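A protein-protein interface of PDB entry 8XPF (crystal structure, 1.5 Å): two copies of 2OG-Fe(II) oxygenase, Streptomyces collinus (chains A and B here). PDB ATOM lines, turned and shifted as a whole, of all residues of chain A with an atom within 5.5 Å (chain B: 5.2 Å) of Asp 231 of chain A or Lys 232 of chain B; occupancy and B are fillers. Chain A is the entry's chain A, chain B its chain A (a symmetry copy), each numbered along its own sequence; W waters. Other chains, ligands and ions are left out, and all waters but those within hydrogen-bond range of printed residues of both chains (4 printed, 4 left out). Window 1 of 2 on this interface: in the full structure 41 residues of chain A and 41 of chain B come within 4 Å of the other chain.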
ATOM      1  N   MET A  91      26.432 -15.147 -31.553  1.00  0.00           N
ATOM      2  CA  MET A  91      27.441 -15.493 -30.558  1.00  0.00           C
ATOM      3  C   MET A  91      27.035 -14.875 -29.222  1.00  0.00           C
ATOM      4  O   MET A  91      26.974 -13.644 -29.087  1.00  0.00           O
ATOM      5  CB  MET A  91      28.823 -15.007 -30.988  1.00  0.00           C
ATOM      6  CG  MET A  91      29.936 -15.533 -30.054  1.00  0.00           C
ATOM      7  SD  MET A  91      31.581 -14.952 -30.532  1.00  0.00           S
ATOM      8  CE  MET A  91      31.497 -13.331 -29.789  1.00  0.00           C
ATOM      9  N   THR A  92      26.750 -15.738 -28.238  1.00  0.00           N
ATOM     10  CA  THR A  92      26.303 -15.308 -26.917  1.00  0.00           C
ATOM     11  C   THR A  92      27.454 -14.775 -26.071  1.00  0.00           C
ATOM     12  O   THR A  92      27.271 -13.854 -25.269  1.00  0.00           O
ATOM     13  CB  THR A  92      25.723 -16.514 -26.186  1.00  0.00           C
ATOM     14  OG1 THR A  92      24.986 -17.329 -27.106  1.00  0.00           O
ATOM     15  CG2 THR A  92      24.823 -16.063 -25.042  1.00  0.00           C
ATOM     16  N   ALA A 118      19.495 -18.052 -20.154  1.00  0.00           N
ATOM     17  CA  ALA A 118      20.022 -16.716 -20.390  1.00  0.00           C
ATOM     18  C   ALA A 118      20.459 -16.089 -19.066  1.00  0.00           C
ATOM     19  O   ALA A 118      20.004 -16.464 -17.985  1.00  0.00           O
ATOM     20  CB  ALA A 118      18.937 -15.854 -21.030  1.00  0.00           C
ATOM     21  N   ALA A 119      21.327 -15.076 -19.170  1.00  0.00           N
ATOM     22  CA  ALA A 119      21.935 -14.477 -17.983  1.00  0.00           C
ATOM     23  C   ALA A 119      20.903 -13.888 -17.029  1.00  0.00           C
ATOM     24  O   ALA A 119      21.085 -13.937 -15.807  1.00  0.00           O
ATOM     25  CB  ALA A 119      22.935 -13.394 -18.397  1.00  0.00           C
ATOM     26  N   SER A 120      19.835 -13.305 -17.562  1.00  0.00           N
ATOM     27  CA  SER A 120      18.814 -12.658 -16.749  1.00  0.00           C
ATOM     28  C   SER A 120      17.768 -13.630 -16.224  1.00  0.00           C
ATOM     29  O   SER A 120      16.896 -13.219 -15.454  1.00  0.00           O
ATOM     30  CB  SER A 120      18.063 -11.644 -17.605  1.00  0.00           C
ATOM     31  OG  SER A 120      17.378 -12.346 -18.633  1.00  0.00           O
ATOM     32  N   HIS A 223      23.625 -19.046 -29.663  1.00  0.00           N
ATOM     33  CA  HIS A 223      22.194 -19.266 -29.485  1.00  0.00           C
ATOM     34  C   HIS A 223      21.464 -18.827 -30.751  1.00  0.00           C
ATOM     35  O   HIS A 223      22.047 -18.197 -31.643  1.00  0.00           O
ATOM     36  CB  HIS A 223      21.658 -18.551 -28.227  1.00  0.00           C
ATOM     37  CG  HIS A 223      21.613 -17.053 -28.343  1.00  0.00           C
ATOM     38  ND1 HIS A 223      22.693 -16.258 -28.031  1.00  0.00           N
ATOM     39  CD2 HIS A 223      20.620 -16.207 -28.724  1.00  0.00           C
ATOM     40  CE1 HIS A 223      22.374 -14.988 -28.220  1.00  0.00           C
ATOM     41  NE2 HIS A 223      21.126 -14.929 -28.655  1.00  0.00           N
ATOM     42  N   ARG A 228      14.821 -14.479 -27.956  1.00  0.00           N
ATOM     43  CA  ARG A 228      15.101 -13.046 -28.045  1.00  0.00           C
ATOM     44  C   ARG A 228      15.416 -12.405 -26.703  1.00  0.00           C
ATOM     45  O   ARG A 228      15.901 -11.263 -26.671  1.00  0.00           O
ATOM     46  CB  ARG A 228      13.905 -12.331 -28.668  1.00  0.00           C
ATOM     47  CG  ARG A 228      12.643 -12.430 -27.816  1.00  0.00           C
ATOM     48  CD  ARG A 228      11.622 -11.408 -28.238  1.00  0.00           C
ATOM     49  NE  ARG A 228      11.144 -11.636 -29.595  1.00  0.00           N
ATOM     50  CZ  ARG A 228      10.418 -10.761 -30.270  1.00  0.00           C
ATOM     51  NH1 ARG A 228      10.103  -9.583 -29.756  1.00  0.00           N
ATOM     52  NH2 ARG A 228      10.009 -11.066 -31.501  1.00  0.00           N
ATOM     53  N   TRP A 229      15.137 -13.087 -25.602  1.00  0.00           N
ATOM     54  CA  TRP A 229      15.491 -12.552 -24.300  1.00  0.00           C
ATOM     55  C   TRP A 229      16.957 -12.793 -23.971  1.00  0.00           C
ATOM     56  O   TRP A 229      17.437 -12.305 -22.945  1.00  0.00           O
ATOM     57  CB  TRP A 229      14.581 -13.172 -23.227  1.00  0.00           C
ATOM     58  CG  TRP A 229      14.853 -14.642 -23.022  1.00  0.00           C
ATOM     59  CD1 TRP A 229      15.700 -15.190 -22.105  1.00  0.00           C
ATOM     60  CD2 TRP A 229      14.336 -15.734 -23.795  1.00  0.00           C
ATOM     61  NE1 TRP A 229      15.734 -16.563 -22.246  1.00  0.00           N
ATOM     62  CE2 TRP A 229      14.905 -16.919 -23.277  1.00  0.00           C
ATOM     63  CE3 TRP A 229      13.442 -15.824 -24.861  1.00  0.00           C
ATOM     64  CZ2 TRP A 229      14.604 -18.182 -23.791  1.00  0.00           C
ATOM     65  CZ3 TRP A 229      13.142 -17.082 -25.372  1.00  0.00           C
ATOM     66  CH2 TRP A 229      13.719 -18.239 -24.838  1.00  0.00           C
ATOM     67  N   THR A 230      17.655 -13.571 -24.796  1.00  0.00           N
ATOM     68  CA  THR A 230      19.072 -13.848 -24.594  1.00  0.00           C
ATOM     69  C   THR A 230      19.898 -12.721 -25.196  1.00  0.00           C
ATOM     70  O   THR A 230      19.588 -12.220 -26.276  1.00  0.00           O
ATOM     71  CB  THR A 230      19.427 -15.152 -25.307  1.00  0.00           C
ATOM     72  OG1 THR A 230      18.477 -16.152 -24.927  1.00  0.00           O
ATOM     73  CG2 THR A 230      20.818 -15.634 -24.934  1.00  0.00           C
ATOM     74  N   ASP A 231      20.971 -12.370 -24.511  1.00  0.00           N
ATOM     75  CA  ASP A 231      21.892 -11.333 -24.950  1.00  0.00           C
ATOM     76  C   ASP A 231      22.975 -11.923 -25.844  1.00  0.00           C
ATOM     77  O   ASP A 231      23.499 -13.002 -25.576  1.00  0.00           O
ATOM     78  CB  ASP A 231      22.549 -10.719 -23.714  1.00  0.00           C
ATOM     79  CG  ASP A 231      21.530 -10.221 -22.702  1.00  0.00           C
ATOM     80  OD1 ASP A 231      20.890  -9.180 -22.981  1.00  0.00           O
ATOM     81  OD2 ASP A 231      21.350 -10.897 -21.654  1.00  0.00           O
ATOM     82  N   LYS A 232      23.310 -11.215 -26.911  1.00  0.00           N
ATOM     83  CA  LYS A 232      24.537 -11.571 -27.598  1.00  0.00           C
ATOM     84  C   LYS A 232      25.722 -10.991 -26.827  1.00  0.00           C
ATOM     85  O   LYS A 232      25.558 -10.220 -25.878  1.00  0.00           O
ATOM     86  CB  LYS A 232      24.495 -11.136 -29.058  1.00  0.00           C
ATOM     87  CG  LYS A 232      24.417  -9.667 -29.254  1.00  0.00           C
ATOM     88  CD  LYS A 232      24.131  -9.333 -30.727  1.00  0.00           C
ATOM     89  CE  LYS A 232      24.068  -7.834 -30.892  1.00  0.00           C
ATOM     90  NZ  LYS A 232      25.364  -7.218 -30.491  1.00  0.00           N
ATOM     91  N   HIS A 233      26.928 -11.398 -27.208  1.00  0.00           N
ATOM     92  CA  HIS A 233      28.101 -11.013 -26.432  1.00  0.00           C
ATOM     93  C   HIS A 233      28.267  -9.491 -26.436  1.00  0.00           C
ATOM     94  O   HIS A 233      28.210  -8.851 -27.492  1.00  0.00           O
ATOM     95  CB  HIS A 233      29.339 -11.680 -27.032  1.00  0.00           C
ATOM     96  CG  HIS A 233      30.601 -11.382 -26.284  1.00  0.00           C
ATOM     97  ND1 HIS A 233      30.783 -11.727 -24.963  1.00  0.00           N
ATOM     98  CD2 HIS A 233      31.737 -10.746 -26.665  1.00  0.00           C
ATOM     99  CE1 HIS A 233      31.979 -11.331 -24.564  1.00  0.00           C
ATOM    100  NE2 HIS A 233      32.576 -10.722 -25.577  1.00  0.00           N
ATOM    101  N   ARG B  90      13.529  -2.032 -27.358  1.00  0.00           N
ATOM    102  CA  ARG B  90      14.278  -2.670 -26.286  1.00  0.00           C
ATOM    103  C   ARG B  90      14.921  -1.621 -25.393  1.00  0.00           C
ATOM    104  O   ARG B  90      15.375  -0.574 -25.871  1.00  0.00           O
ATOM    105  CB  ARG B  90      15.411  -3.549 -26.830  1.00  0.00           C
ATOM    106  CG  ARG B  90      14.997  -4.711 -27.705  1.00  0.00           C
ATOM    107  CD  ARG B  90      14.173  -5.768 -26.951  1.00  0.00           C
ATOM    108  NE  ARG B  90      13.914  -6.890 -27.849  1.00  0.00           N
ATOM    109  CZ  ARG B  90      12.969  -6.894 -28.780  1.00  0.00           C
ATOM    110  NH1 ARG B  90      12.058  -5.939 -28.849  1.00  0.00           N
ATOM    111  NH2 ARG B  90      12.955  -7.868 -29.691  1.00  0.00           N
ATOM    112  N   MET B  91      14.989  -1.919 -24.100  1.00  0.00           N
ATOM    113  CA  MET B  91      15.769  -1.110 -23.170  1.00  0.00           C
ATOM    114  C   MET B  91      17.246  -1.451 -23.353  1.00  0.00           C
ATOM    115  O   MET B  91      17.669  -2.588 -23.099  1.00  0.00           O
ATOM    116  CB  MET B  91      15.327  -1.352 -21.729  1.00  0.00           C
ATOM    117  CG  MET B  91      15.995  -0.366 -20.746  1.00  0.00           C
ATOM    118  SD  MET B  91      15.502  -0.649 -19.029  1.00  0.00           S
ATOM    119  CE  MET B  91      16.606  -2.006 -18.674  1.00  0.00           C
ATOM    120  N   THR B  92      18.026  -0.460 -23.805  1.00  0.00           N
ATOM    121  CA  THR B  92      19.449  -0.637 -24.076  1.00  0.00           C
ATOM    122  C   THR B  92      20.275  -0.658 -22.794  1.00  0.00           C
ATOM    123  O   THR B  92      21.283  -1.366 -22.708  1.00  0.00           O
ATOM    124  CB  THR B  92      19.934   0.545 -24.909  1.00  0.00           C
ATOM    125  OG1 THR B  92      18.929   0.908 -25.863  1.00  0.00           O
ATOM    126  CG2 THR B  92      21.236   0.197 -25.620  1.00  0.00           C
ATOM    127  N   HIS B 223      16.194   1.565 -27.714  1.00  0.00           N
ATOM    128  CA  HIS B 223      16.459   1.483 -29.146  1.00  0.00           C
ATOM    129  C   HIS B 223      15.410   0.585 -29.794  1.00  0.00           C
ATOM    130  O   HIS B 223      14.635  -0.095 -29.108  1.00  0.00           O
ATOM    131  CB  HIS B 223      17.896   1.002 -29.434  1.00  0.00           C
ATOM    132  CG  HIS B 223      18.138  -0.445 -29.108  1.00  0.00           C
ATOM    133  ND1 HIS B 223      18.515  -0.863 -27.851  1.00  0.00           N
ATOM    134  CD2 HIS B 223      18.066  -1.567 -29.872  1.00  0.00           C
ATOM    135  CE1 HIS B 223      18.660  -2.179 -27.849  1.00  0.00           C
ATOM    136  NE2 HIS B 223      18.379  -2.633 -29.059  1.00  0.00           N
ATOM    137  N   THR B 230      22.778  -3.751 -31.920  1.00  0.00           N
ATOM    138  CA  THR B 230      22.766  -3.110 -30.610  1.00  0.00           C
ATOM    139  C   THR B 230      22.363  -4.128 -29.554  1.00  0.00           C
ATOM    140  O   THR B 230      21.466  -4.941 -29.772  1.00  0.00           O
ATOM    141  CB  THR B 230      21.737  -1.980 -30.622  1.00  0.00           C
ATOM    142  OG1 THR B 230      21.968  -1.167 -31.776  1.00  0.00           O
ATOM    143  CG2 THR B 230      21.845  -1.110 -29.382  1.00  0.00           C
ATOM    144  N   ASP B 231      22.999  -4.036 -28.399  1.00  0.00           N
ATOM    145  CA  ASP B 231      22.722  -4.907 -27.267  1.00  0.00           C
ATOM    146  C   ASP B 231      21.610  -4.324 -26.403  1.00  0.00           C
ATOM    147  O   ASP B 231      21.566  -3.121 -26.155  1.00  0.00           O
ATOM    148  CB  ASP B 231      23.994  -5.021 -26.428  1.00  0.00           C
ATOM    149  CG  ASP B 231      25.191  -5.473 -27.247  1.00  0.00           C
ATOM    150  OD1 ASP B 231      25.229  -6.671 -27.617  1.00  0.00           O
ATOM    151  OD2 ASP B 231      26.067  -4.618 -27.548  1.00  0.00           O
ATOM    152  N   LYS B 232      20.710  -5.178 -25.946  1.00  0.00           N
ATOM    153  CA  LYS B 232      19.838  -4.730 -24.876  1.00  0.00           C
ATOM    154  C   LYS B 232      20.599  -4.807 -23.553  1.00  0.00           C
ATOM    155  O   LYS B 232      21.713  -5.332 -23.480  1.00  0.00           O
ATOM    156  CB  LYS B 232      18.531  -5.515 -24.868  1.00  0.00           C
ATOM    157  CG  LYS B 232      18.691  -6.963 -24.583  1.00  0.00           C
ATOM    158  CD  LYS B 232      17.373  -7.712 -24.836  1.00  0.00           C
ATOM    159  CE  LYS B 232      17.569  -9.177 -24.528  1.00  0.00           C
ATOM    160  NZ  LYS B 232      17.969  -9.353 -23.105  1.00  0.00           N
ATOM    161  N   HIS B 233      20.013  -4.239 -22.504  1.00  0.00           N
ATOM    162  CA  HIS B 233      20.735  -4.134 -21.242  1.00  0.00           C
ATOM    163  C   HIS B 233      21.069  -5.526 -20.700  1.00  0.00           C
ATOM    164  O   HIS B 233      20.202  -6.405 -20.638  1.00  0.00           O
ATOM    165  CB  HIS B 233      19.875  -3.369 -20.235  1.00  0.00           C
ATOM    166  CG  HIS B 233      20.540  -3.168 -18.910  1.00  0.00           C
ATOM    167  ND1 HIS B 233      21.719  -2.471 -18.766  1.00  0.00           N
ATOM    168  CD2 HIS B 233      20.205  -3.597 -17.667  1.00  0.00           C
ATOM    169  CE1 HIS B 233      22.077  -2.465 -17.494  1.00  0.00           C
ATOM    170  NE2 HIS B 233      21.178  -3.152 -16.805  1.00  0.00           N
ATOM    171  N   LEU B 234      22.329  -5.718 -20.300  1.00  0.00           N
ATOM    172  CA  LEU B 234      22.808  -7.002 -19.794  1.00  0.00           C
ATOM    173  C   LEU B 234      22.847  -6.988 -18.272  1.00  0.00           C
ATOM    174  O   LEU B 234      23.440  -6.086 -17.662  1.00  0.00           O
ATOM    175  CB  LEU B 234      24.212  -7.273 -20.335  1.00  0.00           C
ATOM    176  CG  LEU B 234      24.965  -8.498 -19.816  1.00  0.00           C
ATOM    177  CD1 LEU B 234      24.178  -9.746 -20.135  1.00  0.00           C
ATOM    178  CD2 LEU B 234      26.357  -8.569 -20.445  1.00  0.00           C
ATOM    179  N   TRP B 235      22.243  -8.010 -17.660  1.00  0.00           N
ATOM    180  CA  TRP B 235      22.374  -8.245 -16.231  1.00  0.00           C
ATOM    181  C   TRP B 235      22.274  -9.738 -15.957  1.00  0.00           C
ATOM    182  O   TRP B 235      21.788 -10.502 -16.789  1.00  0.00           O
ATOM    183  CB  TRP B 235      21.324  -7.474 -15.417  1.00  0.00           C
ATOM    184  CG  TRP B 235      19.919  -8.026 -15.463  1.00  0.00           C
ATOM    185  CD1 TRP B 235      19.350  -8.908 -14.575  1.00  0.00           C
ATOM    186  CD2 TRP B 235      18.906  -7.714 -16.422  1.00  0.00           C
ATOM    187  NE1 TRP B 235      18.051  -9.143 -14.932  1.00  0.00           N
ATOM    188  CE2 TRP B 235      17.750  -8.420 -16.056  1.00  0.00           C
ATOM    189  CE3 TRP B 235      18.857  -6.874 -17.545  1.00  0.00           C
ATOM    190  CZ2 TRP B 235      16.565  -8.353 -16.790  1.00  0.00           C
ATOM    191  CZ3 TRP B 235      17.679  -6.801 -18.270  1.00  0.00           C
ATOM    192  CH2 TRP B 235      16.547  -7.544 -17.888  1.00  0.00           C
ATOM    193  N   LEU B 261      10.107  -4.671 -23.802  1.00  0.00           N
ATOM    194  CA  LEU B 261      11.373  -3.951 -23.870  1.00  0.00           C
ATOM    195  C   LEU B 261      12.513  -4.724 -23.231  1.00  0.00           C
ATOM    196  O   LEU B 261      13.680  -4.408 -23.479  1.00  0.00           O
ATOM    197  CB  LEU B 261      11.257  -2.555 -23.250  1.00  0.00           C
ATOM    198  CG  LEU B 261      10.814  -1.474 -24.241  1.00  0.00           C
ATOM    199  CD1 LEU B 261       9.395  -1.726 -24.727  1.00  0.00           C
ATOM    200  CD2 LEU B 261      10.927  -0.093 -23.596  1.00  0.00           C
ATOM    201  N   LEU B 262      12.207  -5.744 -22.436  1.00  0.00           N
ATOM    202  CA  LEU B 262      13.223  -6.611 -21.858  1.00  0.00           C
ATOM    203  C   LEU B 262      13.508  -7.837 -22.723  1.00  0.00           C
ATOM    204  O   LEU B 262      14.290  -8.704 -22.317  1.00  0.00           O
ATOM    205  CB  LEU B 262      12.791  -7.033 -20.449  1.00  0.00           C
ATOM    206  CG  LEU B 262      12.493  -5.867 -19.505  1.00  0.00           C
ATOM    207  CD1 LEU B 262      12.128  -6.375 -18.114  1.00  0.00           C
ATOM    208  CD2 LEU B 262      13.663  -4.883 -19.424  1.00  0.00           C
ATOM    209  N   GLY B 263      12.907  -7.922 -23.905  1.00  0.00           N
ATOM    210  CA  GLY B 263      13.074  -9.096 -24.740  1.00  0.00           C
ATOM    211  C   GLY B 263      12.135 -10.223 -24.394  1.00  0.00           C
ATOM    212  O   GLY B 263      12.355 -11.366 -24.815  1.00  0.00           O
HETATM  213  O   HOH W   1      16.297 -11.069 -14.076  1.00  0.00           O
HETATM  214  O   HOH W   2      15.769  -8.983 -28.260  1.00  0.00           O
HETATM  215  O   HOH W   3      16.374 -10.344 -21.167  1.00  0.00           O
HETATM  216  O   HOH W   4      20.467  -9.737 -19.345  1.00  0.00           O
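NZ of Lys 232 of chain A lies within salt-bridge range of OD1 of Asp 231 of chain B, at 2.9 Å.
The guanidinium group of Arg 90 of chain B lies close to the guanidinium group of Arg 228 of chain A.
The side-chain carboxylate of Asp 231 of chain A is in salt-bridge range of the side-chain amino group of Lys 232 of chain B, 2.9 Å away.
O of Trp 229 of chain A is in hydrogen-bond range of NZ of Lys 232 of chain B.
N of Trp 229 of chain A sits close to O of Gly 263 of chain B (3.4 Å).
The backbone carbonyl oxygen (O) of Met 91 of chain A sits at hydrogen-bond distance from the backbone NH (N) of His 233 of chain A (2.9 Å).
The backbone NH (N) of Arg 90 of chain B is in hydrogen-bond range of the backbone carbonyl oxygen (O) of His 223 of chain B, at 2.8 Å.
The backbone carbonyl oxygen of Met 91 of chain B lies within hydrogen-bond range of the backbone NH of His 233 of chain B (2.9 Å).
The backbone carbonyl oxygen (O) of Thr 92 of chain A sits at hydrogen-bond distance from the backbone NH (N) of His 233 of chain A, at 3.1 Å.
The backbone NH (N) of His 233 of chain B is in hydrogen-bond range of the backbone carbonyl oxygen (O) of Thr 92 of chain B (3.1 Å).
Ala 119 of chain A touches Trp 235 of chain B.
Ser 120 of chain A touches Trp 235 of chain B (N to O, 3.5 Å).
O of Arg 228 of chain A touches CE of Lys 232 of chain B, 3.4 Å away.
Arg 228 of chain A touches Gly 263 of chain B.
Asp 231 of chain A touches His 233 of chain B.
Asp 231 of chain A touches Leu 234 of chain B (OD2 to CD1, 3.4 Å).
Asp 231 of chain B touches His 233 of chain A (OD1 to O, 3.7 Å).
Printed residues of chain B within 4 Å of Trp 229 of chain A: Lys 232 (3.0 Å) and Gly 263 (3.3 Å).
Asp 231 of chain A touches just these residues of chain B: Lys 232, His 233 and Leu 234.
Of the printed residues of chain B, Lys 232 of chain A touches Asp 231 (2.9 Å).
Printed residues of chain B within 4 Å of His 233 of chain A: Asp 231.
Printed residues of chain A within 4 Å of Arg 90 of chain B: Arg 228.
Printed residues of chain A within 4 Å of Asp 231 of chain B: Lys 232 and His 233.
Lys 232 of chain B touches three residues of chain A.
Of the 13 printed residues of chain B, 7 touch a printed residue of chain A.
Hydrophobic or aromatic side chains of chain B that line the printed part of chain A: Leu 234 and Trp 235.
Of the 12 printed residues of chain A, 7 touch a printed residue of chain B.
Hydrophobic or aromatic side chains of chain A that line the printed part of chain B: Ala 119 and Trp 229.
Among the printed residues, Asp or Glu carboxylates within 4 Å of a Lys or Arg side-chain nitrogen of the other chain: Asp 231 of chain A with Lys 232 of chain B and Lys 232 of chain A with Asp 231 of chain B.
Asp 231 of chain A touches Lys 232 of chain B, and with the chains exchanged Lys 232 of chain A touches Asp 231 of chain B.
Asp 231 of chain A touches His 233 of chain B, and with the chains exchanged His 233 of chain A touches Asp 231 of chain B.
7 positions are printed for both chains.
Of the 12 pairs that touch across the chains among the printed residues, 4 have their exchanged pair printed and touching as well.
Water W1 bridges O of Ser 120 of chain A and NE1 of Trp 235 of chain B.
Water W3 lies within hydrogen-bond range of the side-chain amino group of Lys 232 of chain B (2.7 Å), the backbone carbonyl oxygen of Trp 229 of chain A (2.9 Å), the backbone carbonyl oxygen of Leu 262 of chain B (2.9 Å) and the side-chain hydroxyl of Ser 120 of chain A (3.4 Å).
Water W4 lies within hydrogen-bond range of OD2 of Asp 231 of chain A and O of Trp 235 of chain B.
Water W2 lies within hydrogen-bond range of the backbone carbonyl oxygen (O) of Arg 228 of chain A and the guanidinium group (NE) of Arg 90 of chain B.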
